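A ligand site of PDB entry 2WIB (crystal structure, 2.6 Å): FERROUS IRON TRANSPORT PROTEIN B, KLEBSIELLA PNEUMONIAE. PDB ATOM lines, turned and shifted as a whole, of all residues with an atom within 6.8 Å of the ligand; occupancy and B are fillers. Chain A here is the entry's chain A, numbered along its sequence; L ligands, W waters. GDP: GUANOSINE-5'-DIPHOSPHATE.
Water W1 lies within hydrogen-bond range of the side-chain hydroxyl of Thr 17 (2.7 Å), an oxygen (O1B) of the ligand (2.8 Å) and the side-chain amino group of Lys 16 (2.9 Å).
Water W2 lies within hydrogen-bond range of the backbone carbonyl oxygen of Asn 11 and an oxygen (O2B) of the ligand.
NZ of Lys 16 lies within salt-bridge range of OD1 of Asp 56.
The side-chain hydroxyl (OG) of Ser 14 sits at hydrogen-bond distance from the backbone carbonyl oxygen (O) of Asn 11, 2.8 Å away.
ND2 of Asn 120 lies within hydrogen-bond range of OG of Ser 150 (2.9 Å).
N of Met 121 sits at hydrogen-bond distance from O of Leu 148, 3.2 Å away.
The backbone carbonyl oxygen (O) of Ser 14 lies close to the side-chain amide oxygen (OD1) of Asn 120 (2.8 Å).
The side-chain hydroxyl (OG1) of Thr 18 sits at hydrogen-bond distance from an oxygen (O1A) of the ligand (2.8 Å).
The side-chain hydroxyl of Thr 17 is in hydrogen-bond range of an oxygen (O1B) of the ligand (2.7 Å).
N of Gly 15 lies within hydrogen-bond range of O2B of the ligand (3.1 Å).
N of Ser 150 is in hydrogen-bond range of O6 of the ligand, 3.1 Å away.
A nitrogen (N7) of the ligand sits close to the side-chain amide oxygen (OD1) of Asn 120 (3.2 Å).
N of Ser 14 lies within hydrogen-bond range of O2B of the ligand (3.0 Å).
An oxygen (O1A) of the ligand is in hydrogen-bond range of the backbone NH (N) of Thr 18, 2.8 Å away.
The backbone NH (N) of Thr 17 lies within hydrogen-bond range of an oxygen (O1B) of the ligand, at 2.8 Å.
An oxygen (O2B) of the ligand lies within hydrogen-bond range of the backbone NH (N) of Asn 13 (2.9 Å).
N of Met 121 lies within hydrogen-bond range of O6 of the ligand, at 3.1 Å.
The backbone NH of Lys 16 is in hydrogen-bond range of an oxygen (O2B) of the ligand (3.2 Å).
The side-chain carboxylate (OD1) of Asp 123 lies within hydrogen-bond range of a nitrogen (N1) of the ligand, 2.5 Å away.
C of Pro 12 touches O2B of the ligand, 3.9 Å away.
CG1 of Ile 124 touches N2 of the ligand (3.5 Å).
Val 149 touches the ligand (CA to O6, 3.2 Å).
CG2 of Thr 151 touches C4 of the ligand, at 3.3 Å.
Hydrophobic or aromatic side chains within 4 Å of the ligand: Met 121, Ile 124 and Val 149.
14 residues have an atom within 4 Å of the ligand: Pro 12, Asn 13, Ser 14, Gly 15, Lys 16, Thr 17, Thr 18, Asn 120, Met 121, Asp 123, Ile 124, Val 149, Ser 150 and Thr 151.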
ATOM      1  N   GLY A  10      -9.393 -32.207 -20.594  1.00  0.00           N
ATOM      2  CA  GLY A  10     -10.442 -32.331 -19.557  1.00  0.00           C
ATOM      3  C   GLY A  10     -11.065 -33.753 -19.425  1.00  0.00           C
ATOM      4  O   GLY A  10     -11.085 -34.610 -20.365  1.00  0.00           O
ATOM      5  N   ASN A  11     -11.565 -34.013 -18.221  1.00  0.00           N
ATOM      6  CA  ASN A  11     -12.345 -35.120 -18.109  1.00  0.00           C
ATOM      7  C   ASN A  11     -13.510 -35.042 -19.067  1.00  0.00           C
ATOM      8  O   ASN A  11     -13.973 -33.905 -19.422  1.00  0.00           O
ATOM      9  CB  ASN A  11     -12.881 -35.048 -16.707  1.00  0.00           C
ATOM     10  CG  ASN A  11     -11.822 -35.308 -15.728  1.00  0.00           C
ATOM     11  OD1 ASN A  11     -10.617 -35.482 -16.124  1.00  0.00           O
ATOM     12  ND2 ASN A  11     -12.193 -35.322 -14.450  1.00  0.00           N
ATOM     13  N   PRO A  12     -14.027 -36.229 -19.513  1.00  0.00           N
ATOM     14  CA  PRO A  12     -15.339 -36.180 -20.248  1.00  0.00           C
ATOM     15  C   PRO A  12     -16.382 -35.460 -19.373  1.00  0.00           C
ATOM     16  O   PRO A  12     -16.356 -35.674 -18.140  1.00  0.00           O
ATOM     17  CB  PRO A  12     -15.773 -37.637 -20.376  1.00  0.00           C
ATOM     18  CG  PRO A  12     -14.543 -38.554 -20.014  1.00  0.00           C
ATOM     19  CD  PRO A  12     -13.440 -37.602 -19.426  1.00  0.00           C
ATOM     20  N   ASN A  13     -17.262 -34.636 -19.959  1.00  0.00           N
ATOM     21  CA  ASN A  13     -18.348 -33.999 -19.305  1.00  0.00           C
ATOM     22  C   ASN A  13     -17.982 -32.812 -18.390  1.00  0.00           C
ATOM     23  O   ASN A  13     -18.746 -32.470 -17.448  1.00  0.00           O
ATOM     24  CB  ASN A  13     -19.182 -34.940 -18.521  1.00  0.00           C
ATOM     25  CG  ASN A  13     -19.848 -36.080 -19.422  1.00  0.00           C
ATOM     26  OD1 ASN A  13     -20.306 -35.887 -20.608  1.00  0.00           O
ATOM     27  ND2 ASN A  13     -19.842 -37.289 -18.845  1.00  0.00           N
ATOM     28  N   SER A  14     -16.894 -32.111 -18.768  1.00  0.00           N
ATOM     29  CA  SER A  14     -16.414 -31.016 -18.014  1.00  0.00           C
ATOM     30  C   SER A  14     -16.815 -29.738 -18.704  1.00  0.00           C
ATOM     31  O   SER A  14     -16.538 -28.597 -18.165  1.00  0.00           O
ATOM     32  CB  SER A  14     -14.888 -31.070 -17.842  1.00  0.00           C
ATOM     33  OG  SER A  14     -14.354 -31.153 -19.139  1.00  0.00           O
ATOM     34  N   GLY A  15     -17.470 -29.927 -19.850  1.00  0.00           N
ATOM     35  CA  GLY A  15     -18.082 -28.817 -20.539  1.00  0.00           C
ATOM     36  C   GLY A  15     -17.045 -28.432 -21.595  1.00  0.00           C
ATOM     37  O   GLY A  15     -17.080 -27.306 -22.131  1.00  0.00           O
ATOM     38  N   LYS A  16     -16.115 -29.317 -21.951  1.00  0.00           N
ATOM     39  CA  LYS A  16     -15.134 -28.959 -23.049  1.00  0.00           C
ATOM     40  C   LYS A  16     -15.640 -28.557 -24.414  1.00  0.00           C
ATOM     41  O   LYS A  16     -15.082 -27.734 -25.108  1.00  0.00           O
ATOM     42  CB  LYS A  16     -14.108 -30.036 -23.203  1.00  0.00           C
ATOM     43  CG  LYS A  16     -13.082 -29.773 -24.137  1.00  0.00           C
ATOM     44  CD  LYS A  16     -11.828 -30.459 -23.644  1.00  0.00           C
ATOM     45  CE  LYS A  16     -11.978 -31.945 -23.784  1.00  0.00           C
ATOM     46  NZ  LYS A  16     -12.590 -32.349 -25.204  1.00  0.00           N
ATOM     47  N   THR A  17     -16.721 -29.087 -24.868  1.00  0.00           N
ATOM     48  CA  THR A  17     -17.173 -28.666 -26.197  1.00  0.00           C
ATOM     49  C   THR A  17     -17.744 -27.310 -26.087  1.00  0.00           C
ATOM     50  O   THR A  17     -17.626 -26.506 -27.019  1.00  0.00           O
ATOM     51  CB  THR A  17     -18.252 -29.600 -26.588  1.00  0.00           C
ATOM     52  OG1 THR A  17     -17.623 -30.873 -26.753  1.00  0.00           O
ATOM     53  CG2 THR A  17     -19.077 -29.093 -27.796  1.00  0.00           C
ATOM     54  N   THR A  18     -18.541 -27.133 -25.042  1.00  0.00           N
ATOM     55  CA  THR A  18     -19.194 -25.821 -24.884  1.00  0.00           C
ATOM     56  C   THR A  18     -18.158 -24.724 -25.055  1.00  0.00           C
ATOM     57  O   THR A  18     -18.366 -23.716 -25.805  1.00  0.00           O
ATOM     58  CB  THR A  18     -19.980 -25.714 -23.567  1.00  0.00           C
ATOM     59  OG1 THR A  18     -20.852 -26.875 -23.441  1.00  0.00           O
ATOM     60  CG2 THR A  18     -20.759 -24.406 -23.555  1.00  0.00           C
ATOM     61  N   LEU A  19     -17.031 -24.981 -24.401  1.00  0.00           N
ATOM     62  CA  LEU A  19     -15.909 -24.034 -24.264  1.00  0.00           C
ATOM     63  C   LEU A  19     -15.211 -23.813 -25.583  1.00  0.00           C
ATOM     64  O   LEU A  19     -15.091 -22.664 -26.049  1.00  0.00           O
ATOM     65  CB  LEU A  19     -14.873 -24.545 -23.245  1.00  0.00           C
ATOM     66  CG  LEU A  19     -13.719 -23.529 -23.022  1.00  0.00           C
ATOM     67  CD1 LEU A  19     -14.329 -22.276 -22.749  1.00  0.00           C
ATOM     68  CD2 LEU A  19     -12.900 -24.042 -21.892  1.00  0.00           C
ATOM     69  N   ASP A  56      -8.645 -29.403 -29.896  1.00  0.00           N
ATOM     70  CA  ASP A  56      -9.477 -30.161 -28.940  1.00  0.00           C
ATOM     71  C   ASP A  56      -8.937 -31.523 -28.793  1.00  0.00           C
ATOM     72  O   ASP A  56      -8.520 -32.072 -29.792  1.00  0.00           O
ATOM     73  CB  ASP A  56     -10.844 -30.331 -29.522  1.00  0.00           C
ATOM     74  CG  ASP A  56     -11.736 -31.118 -28.621  1.00  0.00           C
ATOM     75  OD1 ASP A  56     -11.686 -30.978 -27.428  1.00  0.00           O
ATOM     76  OD2 ASP A  56     -12.510 -31.934 -29.116  1.00  0.00           O
ATOM     77  N   GLY A  59     -11.584 -36.357 -24.295  1.00  0.00           N
ATOM     78  CA  GLY A  59     -11.739 -36.457 -22.843  1.00  0.00           C
ATOM     79  C   GLY A  59     -11.021 -37.682 -22.332  1.00  0.00           C
ATOM     80  O   GLY A  59     -11.063 -38.763 -23.001  1.00  0.00           O
ATOM     81  N   VAL A  92      -9.754 -27.939 -18.737  1.00  0.00           N
ATOM     82  CA  VAL A  92     -11.180 -27.664 -18.354  1.00  0.00           C
ATOM     83  C   VAL A  92     -11.575 -28.491 -17.126  1.00  0.00           C
ATOM     84  O   VAL A  92     -11.542 -29.660 -17.156  1.00  0.00           O
ATOM     85  CB  VAL A  92     -12.123 -28.161 -19.425  1.00  0.00           C
ATOM     86  CG1 VAL A  92     -13.514 -27.396 -19.404  1.00  0.00           C
ATOM     87  CG2 VAL A  92     -11.485 -28.134 -20.784  1.00  0.00           C
ATOM     88  N   LEU A 119     -11.782 -23.363 -14.794  1.00  0.00           N
ATOM     89  CA  LEU A 119     -12.681 -23.875 -13.753  1.00  0.00           C
ATOM     90  C   LEU A 119     -14.133 -23.649 -14.237  1.00  0.00           C
ATOM     91  O   LEU A 119     -14.745 -22.559 -14.059  1.00  0.00           O
ATOM     92  CB  LEU A 119     -12.411 -23.228 -12.359  1.00  0.00           C
ATOM     93  CG  LEU A 119     -12.911 -23.957 -11.090  1.00  0.00           C
ATOM     94  CD1 LEU A 119     -12.427 -25.388 -10.890  1.00  0.00           C
ATOM     95  CD2 LEU A 119     -12.361 -23.231  -9.928  1.00  0.00           C
ATOM     96  N   ASN A 120     -14.635 -24.664 -14.931  1.00  0.00           N
ATOM     97  CA  ASN A 120     -15.939 -24.528 -15.614  1.00  0.00           C
ATOM     98  C   ASN A 120     -17.059 -24.986 -14.682  1.00  0.00           C
ATOM     99  O   ASN A 120     -16.804 -25.770 -13.733  1.00  0.00           O
ATOM    100  CB  ASN A 120     -15.959 -25.440 -16.745  1.00  0.00           C
ATOM    101  CG  ASN A 120     -16.968 -25.092 -17.675  1.00  0.00           C
ATOM    102  OD1 ASN A 120     -17.533 -25.965 -18.409  1.00  0.00           O
ATOM    103  ND2 ASN A 120     -17.220 -23.824 -17.746  1.00  0.00           N
ATOM    104  N   MET A 121     -18.290 -24.524 -14.944  1.00  0.00           N
ATOM    105  CA  MET A 121     -19.445 -25.060 -14.154  1.00  0.00           C
ATOM    106  C   MET A 121     -19.471 -24.492 -12.753  1.00  0.00           C
ATOM    107  O   MET A 121     -19.996 -25.147 -11.825  1.00  0.00           O
ATOM    108  CB  MET A 121     -19.533 -26.602 -14.140  1.00  0.00           C
ATOM    109  CG  MET A 121     -19.966 -27.178 -15.534  1.00  0.00           C
ATOM    110  SD  MET A 121     -19.590 -28.969 -15.743  1.00  0.00           S
ATOM    111  CE  MET A 121     -20.200 -29.392 -17.388  1.00  0.00           C
ATOM    112  N   LEU A 122     -18.903 -23.265 -12.603  1.00  0.00           N
ATOM    113  CA  LEU A 122     -19.077 -22.529 -11.380  1.00  0.00           C
ATOM    114  C   LEU A 122     -20.470 -22.376 -10.915  1.00  0.00           C
ATOM    115  O   LEU A 122     -20.663 -22.526  -9.696  1.00  0.00           O
ATOM    116  CB  LEU A 122     -18.241 -21.243 -11.251  1.00  0.00           C
ATOM    117  CG  LEU A 122     -16.780 -21.579 -11.010  1.00  0.00           C
ATOM    118  CD1 LEU A 122     -15.820 -20.411 -11.422  1.00  0.00           C
ATOM    119  CD2 LEU A 122     -16.637 -22.175  -9.641  1.00  0.00           C
ATOM    120  N   ASP A 123     -21.444 -22.144 -11.808  1.00  0.00           N
ATOM    121  CA  ASP A 123     -22.902 -22.310 -11.437  1.00  0.00           C
ATOM    122  C   ASP A 123     -23.395 -23.681 -10.939  1.00  0.00           C
ATOM    123  O   ASP A 123     -24.307 -23.810 -10.088  1.00  0.00           O
ATOM    124  CB  ASP A 123     -23.784 -21.969 -12.652  1.00  0.00           C
ATOM    125  CG  ASP A 123     -23.549 -22.951 -13.886  1.00  0.00           C
ATOM    126  OD1 ASP A 123     -22.391 -23.380 -14.205  1.00  0.00           O
ATOM    127  OD2 ASP A 123     -24.554 -23.205 -14.550  1.00  0.00           O
ATOM    128  N   ILE A 124     -22.896 -24.777 -11.500  1.00  0.00           N
ATOM    129  CA  ILE A 124     -23.370 -26.042 -10.963  1.00  0.00           C
ATOM    130  C   ILE A 124     -22.810 -26.106  -9.525  1.00  0.00           C
ATOM    131  O   ILE A 124     -23.503 -26.559  -8.601  1.00  0.00           O
ATOM    132  CB  ILE A 124     -22.907 -27.284 -11.804  1.00  0.00           C
ATOM    133  CG1 ILE A 124     -23.218 -27.088 -13.283  1.00  0.00           C
ATOM    134  CG2 ILE A 124     -23.523 -28.602 -11.247  1.00  0.00           C
ATOM    135  CD1 ILE A 124     -23.228 -28.439 -14.128  1.00  0.00           C
ATOM    136  N   LEU A 148     -15.164 -20.080 -14.933  1.00  0.00           N
ATOM    137  CA  LEU A 148     -16.003 -20.108 -16.174  1.00  0.00           C
ATOM    138  C   LEU A 148     -17.455 -20.587 -15.959  1.00  0.00           C
ATOM    139  O   LEU A 148     -17.746 -21.359 -15.093  1.00  0.00           O
ATOM    140  CB  LEU A 148     -15.326 -20.902 -17.281  1.00  0.00           C
ATOM    141  CG  LEU A 148     -14.413 -20.114 -18.232  1.00  0.00           C
ATOM    142  CD1 LEU A 148     -13.125 -19.941 -17.631  1.00  0.00           C
ATOM    143  CD2 LEU A 148     -14.096 -20.890 -19.381  1.00  0.00           C
ATOM    144  N   VAL A 149     -18.404 -20.021 -16.669  1.00  0.00           N
ATOM    145  CA  VAL A 149     -19.610 -20.744 -16.934  1.00  0.00           C
ATOM    146  C   VAL A 149     -19.838 -20.738 -18.421  1.00  0.00           C
ATOM    147  O   VAL A 149     -20.265 -19.751 -19.050  1.00  0.00           O
ATOM    148  CB  VAL A 149     -20.845 -20.343 -16.109  1.00  0.00           C
ATOM    149  CG1 VAL A 149     -20.580 -19.364 -15.068  1.00  0.00           C
ATOM    150  CG2 VAL A 149     -22.036 -20.021 -17.036  1.00  0.00           C
ATOM    151  N   SER A 150     -19.406 -21.822 -19.020  1.00  0.00           N
ATOM    152  CA  SER A 150     -19.284 -21.847 -20.549  1.00  0.00           C
ATOM    153  C   SER A 150     -20.561 -21.644 -21.322  1.00  0.00           C
ATOM    154  O   SER A 150     -20.580 -21.035 -22.414  1.00  0.00           O
ATOM    155  CB  SER A 150     -18.569 -23.082 -20.989  1.00  0.00           C
ATOM    156  OG  SER A 150     -17.257 -22.927 -20.502  1.00  0.00           O
ATOM    157  N   THR A 151     -21.639 -22.066 -20.676  1.00  0.00           N
ATOM    158  CA  THR A 151     -23.003 -21.960 -21.217  1.00  0.00           C
ATOM    159  C   THR A 151     -23.374 -20.527 -21.422  1.00  0.00           C
ATOM    160  O   THR A 151     -23.851 -20.097 -22.482  1.00  0.00           O
ATOM    161  CB  THR A 151     -24.035 -22.685 -20.349  1.00  0.00           C
ATOM    162  OG1 THR A 151     -23.913 -22.323 -18.984  1.00  0.00           O
ATOM    163  CG2 THR A 151     -23.957 -24.192 -20.519  1.00  0.00           C
ATOM    164  N   ARG A 152     -23.063 -19.725 -20.389  1.00  0.00           N
ATOM    165  CA  ARG A 152     -23.276 -18.276 -20.553  1.00  0.00           C
ATOM    166  C   ARG A 152     -22.171 -17.570 -21.252  1.00  0.00           C
ATOM    167  O   ARG A 152     -22.387 -16.597 -22.002  1.00  0.00           O
ATOM    168  CB  ARG A 152     -23.828 -17.593 -19.335  1.00  0.00           C
HETATM  169  PB  GDP L   1     -17.861 -32.322 -22.821  1.00  0.00           P
HETATM  170  O1B GDP L   1     -17.482 -31.682 -24.137  1.00  0.00           O
HETATM  171  O2B GDP L   1     -17.014 -32.403 -21.736  1.00  0.00           O
HETATM  172  O3B GDP L   1     -18.127 -33.922 -23.101  1.00  0.00           O
HETATM  173  O3A GDP L   1     -19.058 -31.594 -22.093  1.00  0.00           O
HETATM  174  PA  GDP L   1     -20.001 -30.572 -22.978  1.00  0.00           P
HETATM  175  O1A GDP L   1     -19.387 -29.274 -23.524  1.00  0.00           O
HETATM  176  O2A GDP L   1     -20.659 -31.525 -24.127  1.00  0.00           O
HETATM  177  O5' GDP L   1     -21.208 -30.122 -22.019  1.00  0.00           O
HETATM  178  C5' GDP L   1     -21.646 -31.008 -20.993  1.00  0.00           C
HETATM  179  C4' GDP L   1     -23.084 -30.519 -20.527  1.00  0.00           C
HETATM  180  O4' GDP L   1     -22.663 -29.466 -19.614  1.00  0.00           O
HETATM  181  C3' GDP L   1     -23.729 -29.846 -21.735  1.00  0.00           C
HETATM  182  O3' GDP L   1     -25.164 -29.926 -21.638  1.00  0.00           O
HETATM  183  C2' GDP L   1     -23.355 -28.428 -21.558  1.00  0.00           C
HETATM  184  O2' GDP L   1     -24.452 -27.655 -21.983  1.00  0.00           O
HETATM  185  C1' GDP L   1     -23.240 -28.251 -20.092  1.00  0.00           C
HETATM  186  N9  GDP L   1     -22.325 -27.269 -19.632  1.00  0.00           N
HETATM  187  C8  GDP L   1     -21.099 -26.933 -20.088  1.00  0.00           C
HETATM  188  N7  GDP L   1     -20.604 -25.917 -19.231  1.00  0.00           N
HETATM  189  C5  GDP L   1     -21.478 -25.588 -18.306  1.00  0.00           C
HETATM  190  C6  GDP L   1     -21.496 -24.637 -17.245  1.00  0.00           C
HETATM  191  O6  GDP L   1     -20.537 -23.845 -16.989  1.00  0.00           O
HETATM  192  N1  GDP L   1     -22.669 -24.683 -16.379  1.00  0.00           N
HETATM  193  C2  GDP L   1     -23.745 -25.550 -16.670  1.00  0.00           C
HETATM  194  N2  GDP L   1     -24.900 -25.554 -15.961  1.00  0.00           N
HETATM  195  N3  GDP L   1     -23.632 -26.393 -17.732  1.00  0.00           N
HETATM  196  C4  GDP L   1     -22.562 -26.457 -18.536  1.00  0.00           C
HETATM  197  O   HOH W   1     -15.368 -32.117 -25.857  1.00  0.00           O
HETATM  198  O   HOH W   2     -14.303 -33.359 -21.934  1.00  0.00           O
